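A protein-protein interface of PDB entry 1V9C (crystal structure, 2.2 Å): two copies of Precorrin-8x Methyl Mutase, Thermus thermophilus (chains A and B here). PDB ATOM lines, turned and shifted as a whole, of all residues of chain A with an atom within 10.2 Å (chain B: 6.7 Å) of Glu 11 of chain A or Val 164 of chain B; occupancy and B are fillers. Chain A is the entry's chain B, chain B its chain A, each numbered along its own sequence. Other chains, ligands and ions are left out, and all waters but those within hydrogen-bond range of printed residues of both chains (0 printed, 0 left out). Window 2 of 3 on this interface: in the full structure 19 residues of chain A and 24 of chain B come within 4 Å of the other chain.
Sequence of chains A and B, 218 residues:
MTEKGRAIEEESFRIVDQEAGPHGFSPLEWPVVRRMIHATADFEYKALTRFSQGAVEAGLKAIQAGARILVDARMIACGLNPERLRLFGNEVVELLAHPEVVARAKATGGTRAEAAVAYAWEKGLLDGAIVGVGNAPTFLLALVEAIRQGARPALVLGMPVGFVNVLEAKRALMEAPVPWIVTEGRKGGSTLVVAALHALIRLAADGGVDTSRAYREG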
ATOM      1  N   GLY A   5      13.413  18.553   2.420  1.00  0.00           N
ATOM      2  CA  GLY A   5      14.162  19.466   1.506  1.00  0.00           C
ATOM      3  C   GLY A   5      14.325  18.871   0.122  1.00  0.00           C
ATOM      4  O   GLY A   5      14.032  19.517  -0.885  1.00  0.00           O
ATOM      5  N   ARG A   6      14.798  17.632   0.070  1.00  0.00           N
ATOM      6  CA  ARG A   6      15.002  16.940  -1.198  1.00  0.00           C
ATOM      7  C   ARG A   6      13.626  16.549  -1.732  1.00  0.00           C
ATOM      8  O   ARG A   6      13.357  16.631  -2.934  1.00  0.00           O
ATOM      9  CB  ARG A   6      15.847  15.679  -0.974  1.00  0.00           C
ATOM     10  CG  ARG A   6      17.145  15.918  -0.202  1.00  0.00           C
ATOM     11  CD  ARG A   6      18.279  16.398  -1.101  1.00  0.00           C
ATOM     12  NE  ARG A   6      19.386  16.956  -0.320  1.00  0.00           N
ATOM     13  CZ  ARG A   6      20.623  17.126  -0.781  1.00  0.00           C
ATOM     14  NH1 ARG A   6      20.926  16.777  -2.025  1.00  0.00           N
ATOM     15  NH2 ARG A   6      21.557  17.653   0.002  1.00  0.00           N
ATOM     16  N   ALA A   7      12.760  16.131  -0.814  1.00  0.00           N
ATOM     17  CA  ALA A   7      11.406  15.713  -1.142  1.00  0.00           C
ATOM     18  C   ALA A   7      10.655  16.810  -1.882  1.00  0.00           C
ATOM     19  O   ALA A   7       9.950  16.544  -2.857  1.00  0.00           O
ATOM     20  CB  ALA A   7      10.665  15.337   0.132  1.00  0.00           C
ATOM     21  N   ILE A   8      10.808  18.043  -1.409  1.00  0.00           N
ATOM     22  CA  ILE A   8      10.144  19.182  -2.023  1.00  0.00           C
ATOM     23  C   ILE A   8      10.546  19.294  -3.492  1.00  0.00           C
ATOM     24  O   ILE A   8       9.688  19.489  -4.354  1.00  0.00           O
ATOM     25  CB  ILE A   8      10.487  20.503  -1.282  1.00  0.00           C
ATOM     26  CG1 ILE A   8      10.054  20.413   0.184  1.00  0.00           C
ATOM     27  CG2 ILE A   8       9.790  21.673  -1.939  1.00  0.00           C
ATOM     28  CD1 ILE A   8       8.579  20.133   0.385  1.00  0.00           C
ATOM     29  N   GLU A   9      11.842  19.153  -3.778  1.00  0.00           N
ATOM     30  CA  GLU A   9      12.328  19.235  -5.155  1.00  0.00           C
ATOM     31  C   GLU A   9      11.743  18.114  -6.007  1.00  0.00           C
ATOM     32  O   GLU A   9      11.351  18.332  -7.158  1.00  0.00           O
ATOM     33  CB  GLU A   9      13.856  19.158  -5.210  1.00  0.00           C
ATOM     34  CG  GLU A   9      14.405  19.307  -6.632  1.00  0.00           C
ATOM     35  CD  GLU A   9      15.905  19.061  -6.739  1.00  0.00           C
ATOM     36  OE1 GLU A   9      16.351  17.931  -6.441  1.00  0.00           O
ATOM     37  OE2 GLU A   9      16.632  20.001  -7.127  1.00  0.00           O
ATOM     38  N   GLU A  10      11.699  16.908  -5.448  1.00  0.00           N
ATOM     39  CA  GLU A  10      11.141  15.774  -6.170  1.00  0.00           C
ATOM     40  C   GLU A  10       9.661  16.065  -6.409  1.00  0.00           C
ATOM     41  O   GLU A  10       9.150  15.845  -7.511  1.00  0.00           O
ATOM     42  CB  GLU A  10      11.299  14.485  -5.362  1.00  0.00           C
ATOM     43  CG  GLU A  10      10.644  13.265  -6.006  1.00  0.00           C
ATOM     44  CD  GLU A  10      11.281  12.866  -7.337  1.00  0.00           C
ATOM     45  OE1 GLU A  10      10.714  11.989  -8.026  1.00  0.00           O
ATOM     46  OE2 GLU A  10      12.348  13.418  -7.690  1.00  0.00           O
ATOM     47  N   GLU A  11       8.989  16.573  -5.374  1.00  0.00           N
ATOM     48  CA  GLU A  11       7.576  16.919  -5.458  1.00  0.00           C
ATOM     49  C   GLU A  11       7.375  17.932  -6.571  1.00  0.00           C
ATOM     50  O   GLU A  11       6.536  17.748  -7.452  1.00  0.00           O
ATOM     51  CB  GLU A  11       7.093  17.534  -4.154  1.00  0.00           C
ATOM     52  CG  GLU A  11       5.630  17.976  -4.172  1.00  0.00           C
ATOM     53  CD  GLU A  11       5.269  18.879  -3.000  1.00  0.00           C
ATOM     54  OE1 GLU A  11       4.075  18.955  -2.640  1.00  0.00           O
ATOM     55  OE2 GLU A  11       6.179  19.530  -2.444  1.00  0.00           O
ATOM     56  N   SER A  12       8.154  19.006  -6.522  1.00  0.00           N
ATOM     57  CA  SER A  12       8.070  20.053  -7.524  1.00  0.00           C
ATOM     58  C   SER A  12       8.269  19.555  -8.950  1.00  0.00           C
ATOM     59  O   SER A  12       7.673  20.101  -9.871  1.00  0.00           O
ATOM     60  CB  SER A  12       9.077  21.157  -7.225  1.00  0.00           C
ATOM     61  OG  SER A  12       8.519  22.101  -6.337  1.00  0.00           O
ATOM     62  N   PHE A  13       9.126  18.548  -9.127  1.00  0.00           N
ATOM     63  CA  PHE A  13       9.377  17.978 -10.446  1.00  0.00           C
ATOM     64  C   PHE A  13       8.132  17.219 -10.894  1.00  0.00           C
ATOM     65  O   PHE A  13       7.775  17.235 -12.072  1.00  0.00           O
ATOM     66  CB  PHE A  13      10.559  17.017 -10.415  1.00  0.00           C
ATOM     67  CG  PHE A  13      11.906  17.694 -10.438  1.00  0.00           C
ATOM     68  CD1 PHE A  13      13.037  17.025  -9.972  1.00  0.00           C
ATOM     69  CD2 PHE A  13      12.046  18.991 -10.907  1.00  0.00           C
ATOM     70  CE1 PHE A  13      14.283  17.648  -9.971  1.00  0.00           C
ATOM     71  CE2 PHE A  13      13.285  19.623 -10.910  1.00  0.00           C
ATOM     72  CZ  PHE A  13      14.404  18.956 -10.443  1.00  0.00           C
ATOM     73  N   ARG A  14       7.497  16.541  -9.946  1.00  0.00           N
ATOM     74  CA  ARG A  14       6.272  15.800 -10.201  1.00  0.00           C
ATOM     75  C   ARG A  14       5.249  16.751 -10.782  1.00  0.00           C
ATOM     76  O   ARG A  14       4.669  16.491 -11.835  1.00  0.00           O
ATOM     77  CB  ARG A  14       5.696  15.229  -8.904  1.00  0.00           C
ATOM     78  CG  ARG A  14       5.949  13.751  -8.692  1.00  0.00           C
ATOM     79  CD  ARG A  14       4.898  13.148  -7.760  1.00  0.00           C
ATOM     80  NE  ARG A  14       5.057  13.541  -6.364  1.00  0.00           N
ATOM     81  CZ  ARG A  14       6.165  13.352  -5.650  1.00  0.00           C
ATOM     82  NH1 ARG A  14       7.228  12.781  -6.201  1.00  0.00           N
ATOM     83  NH2 ARG A  14       6.205  13.712  -4.378  1.00  0.00           N
ATOM     84  N   ILE A  15       5.036  17.853 -10.066  1.00  0.00           N
ATOM     85  CA  ILE A  15       4.073  18.879 -10.447  1.00  0.00           C
ATOM     86  C   ILE A  15       4.282  19.391 -11.869  1.00  0.00           C
ATOM     87  O   ILE A  15       3.318  19.614 -12.598  1.00  0.00           O
ATOM     88  CB  ILE A  15       4.122  20.063  -9.457  1.00  0.00           C
ATOM     89  CG1 ILE A  15       3.677  19.575  -8.073  1.00  0.00           C
ATOM     90  CG2 ILE A  15       3.278  21.235  -9.981  1.00  0.00           C
ATOM     91  CD1 ILE A  15       3.522  20.667  -7.039  1.00  0.00           C
ATOM     92  N   VAL A  16       5.531  19.576 -12.269  1.00  0.00           N
ATOM     93  CA  VAL A  16       5.785  20.044 -13.616  1.00  0.00           C
ATOM     94  C   VAL A  16       5.421  18.948 -14.620  1.00  0.00           C
ATOM     95  O   VAL A  16       4.903  19.233 -15.692  1.00  0.00           O
ATOM     96  CB  VAL A  16       7.238  20.405 -13.843  1.00  0.00           C
ATOM     97  CG1 VAL A  16       7.444  20.712 -15.320  1.00  0.00           C
ATOM     98  CG2 VAL A  16       7.635  21.593 -12.987  1.00  0.00           C
ATOM     99  N   ASP A  17       5.704  17.696 -14.280  1.00  0.00           N
ATOM    100  CA  ASP A  17       5.376  16.615 -15.195  1.00  0.00           C
ATOM    101  C   ASP A  17       3.868  16.500 -15.373  1.00  0.00           C
ATOM    102  O   ASP A  17       3.406  16.145 -16.442  1.00  0.00           O
ATOM    103  CB  ASP A  17       5.941  15.280 -14.708  1.00  0.00           C
ATOM    104  CG  ASP A  17       7.329  15.010 -15.246  1.00  0.00           C
ATOM    105  OD1 ASP A  17       7.645  15.506 -16.347  1.00  0.00           O
ATOM    106  OD2 ASP A  17       8.099  14.289 -14.584  1.00  0.00           O
ATOM    107  N   GLN A  18       3.115  16.825 -14.324  1.00  0.00           N
ATOM    108  CA  GLN A  18       1.659  16.754 -14.349  1.00  0.00           C
ATOM    109  C   GLN A  18       0.981  17.821 -15.190  1.00  0.00           C
ATOM    110  O   GLN A  18      -0.084  17.591 -15.754  1.00  0.00           O
ATOM    111  CB  GLN A  18       1.105  16.877 -12.945  1.00  0.00           C
ATOM    112  CG  GLN A  18       1.182  15.633 -12.132  1.00  0.00           C
ATOM    113  CD  GLN A  18       0.665  15.873 -10.736  1.00  0.00           C
ATOM    114  OE1 GLN A  18       0.192  16.974 -10.426  1.00  0.00           O
ATOM    115  NE2 GLN A  18       0.745  14.851  -9.878  1.00  0.00           N
ATOM    116  N   GLU A  19       1.600  18.990 -15.265  1.00  0.00           N
ATOM    117  CA  GLU A  19       1.013  20.098 -15.991  1.00  0.00           C
ATOM    118  C   GLU A  19       1.715  20.437 -17.298  1.00  0.00           C
ATOM    119  O   GLU A  19       1.440  21.472 -17.906  1.00  0.00           O
ATOM    120  CB  GLU A  19       0.990  21.304 -15.069  1.00  0.00           C
ATOM    121  CG  GLU A  19       0.850  20.911 -13.603  1.00  0.00           C
ATOM    122  CD  GLU A  19       0.712  22.113 -12.703  1.00  0.00           C
ATOM    123  OE1 GLU A  19       1.230  23.181 -13.084  1.00  0.00           O
ATOM    124  OE2 GLU A  19       0.097  21.996 -11.618  1.00  0.00           O
ATOM    125  N   ARG A  34      12.199  19.792 -18.412  1.00  0.00           N
ATOM    126  CA  ARG A  34      11.464  19.780 -17.159  1.00  0.00           C
ATOM    127  C   ARG A  34      12.180  20.694 -16.167  1.00  0.00           C
ATOM    128  O   ARG A  34      11.565  21.558 -15.551  1.00  0.00           O
ATOM    129  CB  ARG A  34      11.418  18.351 -16.601  1.00  0.00           C
ATOM    130  CG  ARG A  34      10.655  18.207 -15.294  1.00  0.00           C
ATOM    131  CD  ARG A  34      11.130  16.995 -14.499  1.00  0.00           C
ATOM    132  NE  ARG A  34      10.750  15.709 -15.074  1.00  0.00           N
ATOM    133  CZ  ARG A  34      11.547  14.642 -15.100  1.00  0.00           C
ATOM    134  NH1 ARG A  34      12.772  14.715 -14.593  1.00  0.00           N
ATOM    135  NH2 ARG A  34      11.113  13.494 -15.609  1.00  0.00           N
ATOM    136  N   HIS A  38      10.901  23.981 -14.375  1.00  0.00           N
ATOM    137  CA  HIS A  38      10.880  24.002 -12.929  1.00  0.00           C
ATOM    138  C   HIS A  38      11.580  25.276 -12.432  1.00  0.00           C
ATOM    139  O   HIS A  38      11.070  25.976 -11.565  1.00  0.00           O
ATOM    140  CB  HIS A  38      11.587  22.771 -12.394  1.00  0.00           C
ATOM    141  CG  HIS A  38      11.663  22.732 -10.901  1.00  0.00           C
ATOM    142  ND1 HIS A  38      12.812  23.040 -10.207  1.00  0.00           N
ATOM    143  CD2 HIS A  38      10.722  22.447  -9.969  1.00  0.00           C
ATOM    144  CE1 HIS A  38      12.576  22.947  -8.911  1.00  0.00           C
ATOM    145  NE2 HIS A  38      11.316  22.590  -8.739  1.00  0.00           N
ATOM    146  N   ALA A  41       9.166  28.253 -13.787  1.00  0.00           N
ATOM    147  CA  ALA A  41       7.716  28.184 -13.632  1.00  0.00           C
ATOM    148  C   ALA A  41       7.169  28.770 -14.940  1.00  0.00           C
ATOM    149  O   ALA A  41       6.123  29.394 -14.957  1.00  0.00           O
ATOM    150  CB  ALA A  41       7.253  29.027 -12.440  1.00  0.00           C
ATOM    151  N   ARG A 202      22.903  15.543 -13.413  1.00  0.00           N
ATOM    152  CA  ARG A 202      22.087  14.523 -12.752  1.00  0.00           C
ATOM    153  C   ARG A 202      21.863  13.299 -13.646  1.00  0.00           C
ATOM    154  O   ARG A 202      21.867  12.176 -13.165  1.00  0.00           O
ATOM    155  CB  ARG A 202      20.734  15.104 -12.342  1.00  0.00           C
ATOM    156  CG  ARG A 202      19.782  14.094 -11.716  1.00  0.00           C
ATOM    157  CD  ARG A 202      20.289  13.637 -10.360  1.00  0.00           C
ATOM    158  NE  ARG A 202      19.393  12.671  -9.728  1.00  0.00           N
ATOM    159  CZ  ARG A 202      18.130  12.916  -9.383  1.00  0.00           C
ATOM    160  NH1 ARG A 202      17.587  14.106  -9.604  1.00  0.00           N
ATOM    161  NH2 ARG A 202      17.406  11.964  -8.812  1.00  0.00           N
ATOM    162  N   SER A 212      14.329  10.512 -11.981  1.00  0.00           N
ATOM    163  CA  SER A 212      13.385  11.493 -11.461  1.00  0.00           C
ATOM    164  C   SER A 212      12.040  11.306 -12.155  1.00  0.00           C
ATOM    165  O   SER A 212      11.425  12.323 -12.540  1.00  0.00           O
ATOM    166  CB  SER A 212      13.898  12.915 -11.714  1.00  0.00           C
ATOM    167  OG  SER A 212      15.147  13.137 -11.083  1.00  0.00           O
ATOM    168  N   PRO B 137      11.018  29.850  -0.590  1.00  0.00           N
ATOM    169  CA  PRO B 137       9.724  30.335  -0.105  1.00  0.00           C
ATOM    170  C   PRO B 137       9.652  30.234   1.420  1.00  0.00           C
ATOM    171  O   PRO B 137       9.109  31.114   2.089  1.00  0.00           O
ATOM    172  CB  PRO B 137       8.727  29.404  -0.789  1.00  0.00           C
ATOM    173  CG  PRO B 137       9.447  28.982  -2.035  1.00  0.00           C
ATOM    174  CD  PRO B 137      10.841  28.732  -1.527  1.00  0.00           C
ATOM    175  N   THR B 138      10.197  29.150   1.965  1.00  0.00           N
ATOM    176  CA  THR B 138      10.192  28.957   3.410  1.00  0.00           C
ATOM    177  C   THR B 138      10.890  30.138   4.070  1.00  0.00           C
ATOM    178  O   THR B 138      10.408  30.666   5.066  1.00  0.00           O
ATOM    179  CB  THR B 138      10.925  27.650   3.842  1.00  0.00           C
ATOM    180  OG1 THR B 138      12.313  27.731   3.489  1.00  0.00           O
ATOM    181  CG2 THR B 138      10.289  26.426   3.178  1.00  0.00           C
ATOM    182  N   VAL B 161      10.575  31.746  -7.055  1.00  0.00           N
ATOM    183  CA  VAL B 161      10.015  31.058  -8.220  1.00  0.00           C
ATOM    184  C   VAL B 161       9.752  29.680  -7.657  1.00  0.00           C
ATOM    185  O   VAL B 161      10.511  29.212  -6.811  1.00  0.00           O
ATOM    186  CB  VAL B 161      11.041  30.965  -9.421  1.00  0.00           C
ATOM    187  CG1 VAL B 161      12.313  30.266  -8.974  1.00  0.00           C
ATOM    188  CG2 VAL B 161      10.424  30.190 -10.622  1.00  0.00           C
ATOM    189  N   GLY B 162       8.675  29.034  -8.086  1.00  0.00           N
ATOM    190  CA  GLY B 162       8.400  27.707  -7.569  1.00  0.00           C
ATOM    191  C   GLY B 162       6.957  27.232  -7.599  1.00  0.00           C
ATOM    192  O   GLY B 162       6.034  27.973  -7.973  1.00  0.00           O
ATOM    193  N   PHE B 163       6.783  25.991  -7.149  1.00  0.00           N
ATOM    194  CA  PHE B 163       5.504  25.293  -7.128  1.00  0.00           C
ATOM    195  C   PHE B 163       4.930  24.906  -5.762  1.00  0.00           C
ATOM    196  O   PHE B 163       3.745  24.554  -5.656  1.00  0.00           O
ATOM    197  CB  PHE B 163       5.643  24.051  -7.989  1.00  0.00           C
ATOM    198  CG  PHE B 163       5.983  24.357  -9.414  1.00  0.00           C
ATOM    199  CD1 PHE B 163       4.985  24.724 -10.317  1.00  0.00           C
ATOM    200  CD2 PHE B 163       7.305  24.355  -9.837  1.00  0.00           C
ATOM    201  CE1 PHE B 163       5.296  25.092 -11.618  1.00  0.00           C
ATOM    202  CE2 PHE B 163       7.634  24.724 -11.145  1.00  0.00           C
ATOM    203  CZ  PHE B 163       6.628  25.092 -12.034  1.00  0.00           C
ATOM    204  N   VAL B 164       5.754  24.961  -4.723  1.00  0.00           N
ATOM    205  CA  VAL B 164       5.296  24.606  -3.385  1.00  0.00           C
ATOM    206  C   VAL B 164       5.717  25.704  -2.419  1.00  0.00           C
ATOM    207  O   VAL B 164       6.875  26.148  -2.440  1.00  0.00           O
ATOM    208  CB  VAL B 164       5.926  23.274  -2.883  1.00  0.00           C
ATOM    209  CG1 VAL B 164       5.069  22.689  -1.770  1.00  0.00           C
ATOM    210  CG2 VAL B 164       6.089  22.280  -4.028  1.00  0.00           C
ATOM    211  N   ASN B 165       4.773  26.151  -1.591  1.00  0.00           N
ATOM    212  CA  ASN B 165       5.057  27.181  -0.594  1.00  0.00           C
ATOM    213  C   ASN B 165       5.287  28.573  -1.172  1.00  0.00           C
ATOM    214  O   ASN B 165       5.644  29.491  -0.437  1.00  0.00           O
ATOM    215  CB  ASN B 165       6.300  26.792   0.219  1.00  0.00           C
ATOM    216  CG  ASN B 165       6.159  25.445   0.907  1.00  0.00           C
ATOM    217  OD1 ASN B 165       7.143  24.875   1.381  1.00  0.00           O
ATOM    218  ND2 ASN B 165       4.934  24.935   0.975  1.00  0.00           N
ATOM    219  N   VAL B 166       5.093  28.742  -2.477  1.00  0.00           N
ATOM    220  CA  VAL B 166       5.333  30.043  -3.094  1.00  0.00           C
ATOM    221  C   VAL B 166       4.126  30.975  -3.063  1.00  0.00           C
ATOM    222  O   VAL B 166       4.279  32.175  -2.837  1.00  0.00           O
ATOM    223  CB  VAL B 166       5.832  29.884  -4.554  1.00  0.00           C
ATOM    224  CG1 VAL B 166       6.041  31.231  -5.182  1.00  0.00           C
ATOM    225  CG2 VAL B 166       7.136  29.108  -4.574  1.00  0.00           C
ATOM    226  N   LEU B 167       2.930  30.441  -3.281  1.00  0.00           N
ATOM    227  CA  LEU B 167       1.738  31.288  -3.252  1.00  0.00           C
ATOM    228  C   LEU B 167       1.469  31.825  -1.853  1.00  0.00           C
ATOM    229  O   LEU B 167       1.141  32.998  -1.683  1.00  0.00           O
ATOM    230  CB  LEU B 167       0.499  30.531  -3.739  1.00  0.00           C
ATOM    231  CG  LEU B 167       0.389  30.199  -5.228  1.00  0.00           C
ATOM    232  CD1 LEU B 167      -1.009  29.676  -5.521  1.00  0.00           C
ATOM    233  CD2 LEU B 167       0.676  31.440  -6.063  1.00  0.00           C
ATOM    234  N   ARG B 186       3.491  31.766  -9.470  1.00  0.00           N
ATOM    235  CA  ARG B 186       4.631  30.865  -9.349  1.00  0.00           C
ATOM    236  C   ARG B 186       5.936  31.414  -9.935  1.00  0.00           C
ATOM    237  O   ARG B 186       7.011  30.880  -9.669  1.00  0.00           O
ATOM    238  CB  ARG B 186       4.287  29.550 -10.039  1.00  0.00           C
ATOM    239  CG  ARG B 186       3.324  28.657  -9.251  1.00  0.00           C
ATOM    240  CD  ARG B 186       2.770  27.558 -10.132  1.00  0.00           C
ATOM    241  NE  ARG B 186       2.454  26.329  -9.409  1.00  0.00           N
ATOM    242  CZ  ARG B 186       1.616  26.233  -8.376  1.00  0.00           C
ATOM    243  NH1 ARG B 186       0.978  27.306  -7.914  1.00  0.00           N
ATOM    244  NH2 ARG B 186       1.422  25.051  -7.796  1.00  0.00           N
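The backbone carbonyl oxygen of Arg 186 of chain B lies within hydrogen-bond range of the backbone NH of Gly 162 of chain B (2.9 Å). The backbone carbonyl oxygen of Phe 163 of chain B is in hydrogen-bond range of the guanidinium group of Arg 186 of chain B, 3.2 Å away. The backbone carbonyl oxygen (O) of Ile 8 of chain A lies close to the side-chain hydroxyl (OG) of Ser 12 of chain A (3.5 Å).
Of the 10 printed residues of chain B, 4 touch a printed residue of chain A. Printed residues of chain B that touch a printed residue of chain A: Val 161, Phe 163, Val 164 and Arg 186. Hydrophobic or aromatic side chains of chain B within 4 Å of the printed part of chain A: Val 161, Phe 163 and Val 164. Of the 20 printed residues of chain A, 6 touch a printed residue of chain B.
No position is printed for both chains.
Glu 11 of chain A touches one residue of chain B. Val 164 of chain B touches just these residues of chain A: Glu 11 and Ser 12. Gly 162 of chain B touches none of the printed residues of chain A. Printed residues of chain B within 4 Å of Ile 15 of chain A: Phe 163 (3.9 Å). Of the printed residues of chain B, His 38 of chain A touches Phe 163. Printed residues of chain B within 4 Å of Ser 12 of chain A: Phe 163 (3.8 Å) and Val 164 (3.4 Å). Val 166 of chain B touches none of the printed residues of chain A. The nearest residue of chain B that does not touch Glu 11 of chain A is Phe 163 of chain B (6.4 Å).
Among the printed residues, pairs that only touch across the chains: Glu 11 of chain A with Val 164 of chain B (3.2 Å), Ser 12 of chain A with Phe 163 of chain B (3.8 Å), Ser 12 of chain A with Val 164 of chain B (3.4 Å), Ile 15 of chain A with Phe 163 of chain B (3.9 Å), Val 16 of chain A with Phe 163 of chain B (3.6 Å), His 38 of chain A with Phe 163 of chain B (3.7 Å), Ala 41 of chain A with Val 161 of chain B (3.8 Å), Ala 41 of chain A with Phe 163 of chain B (3.6 Å) and Ala 41 of chain A with Arg 186 of chain B (3.3 Å).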
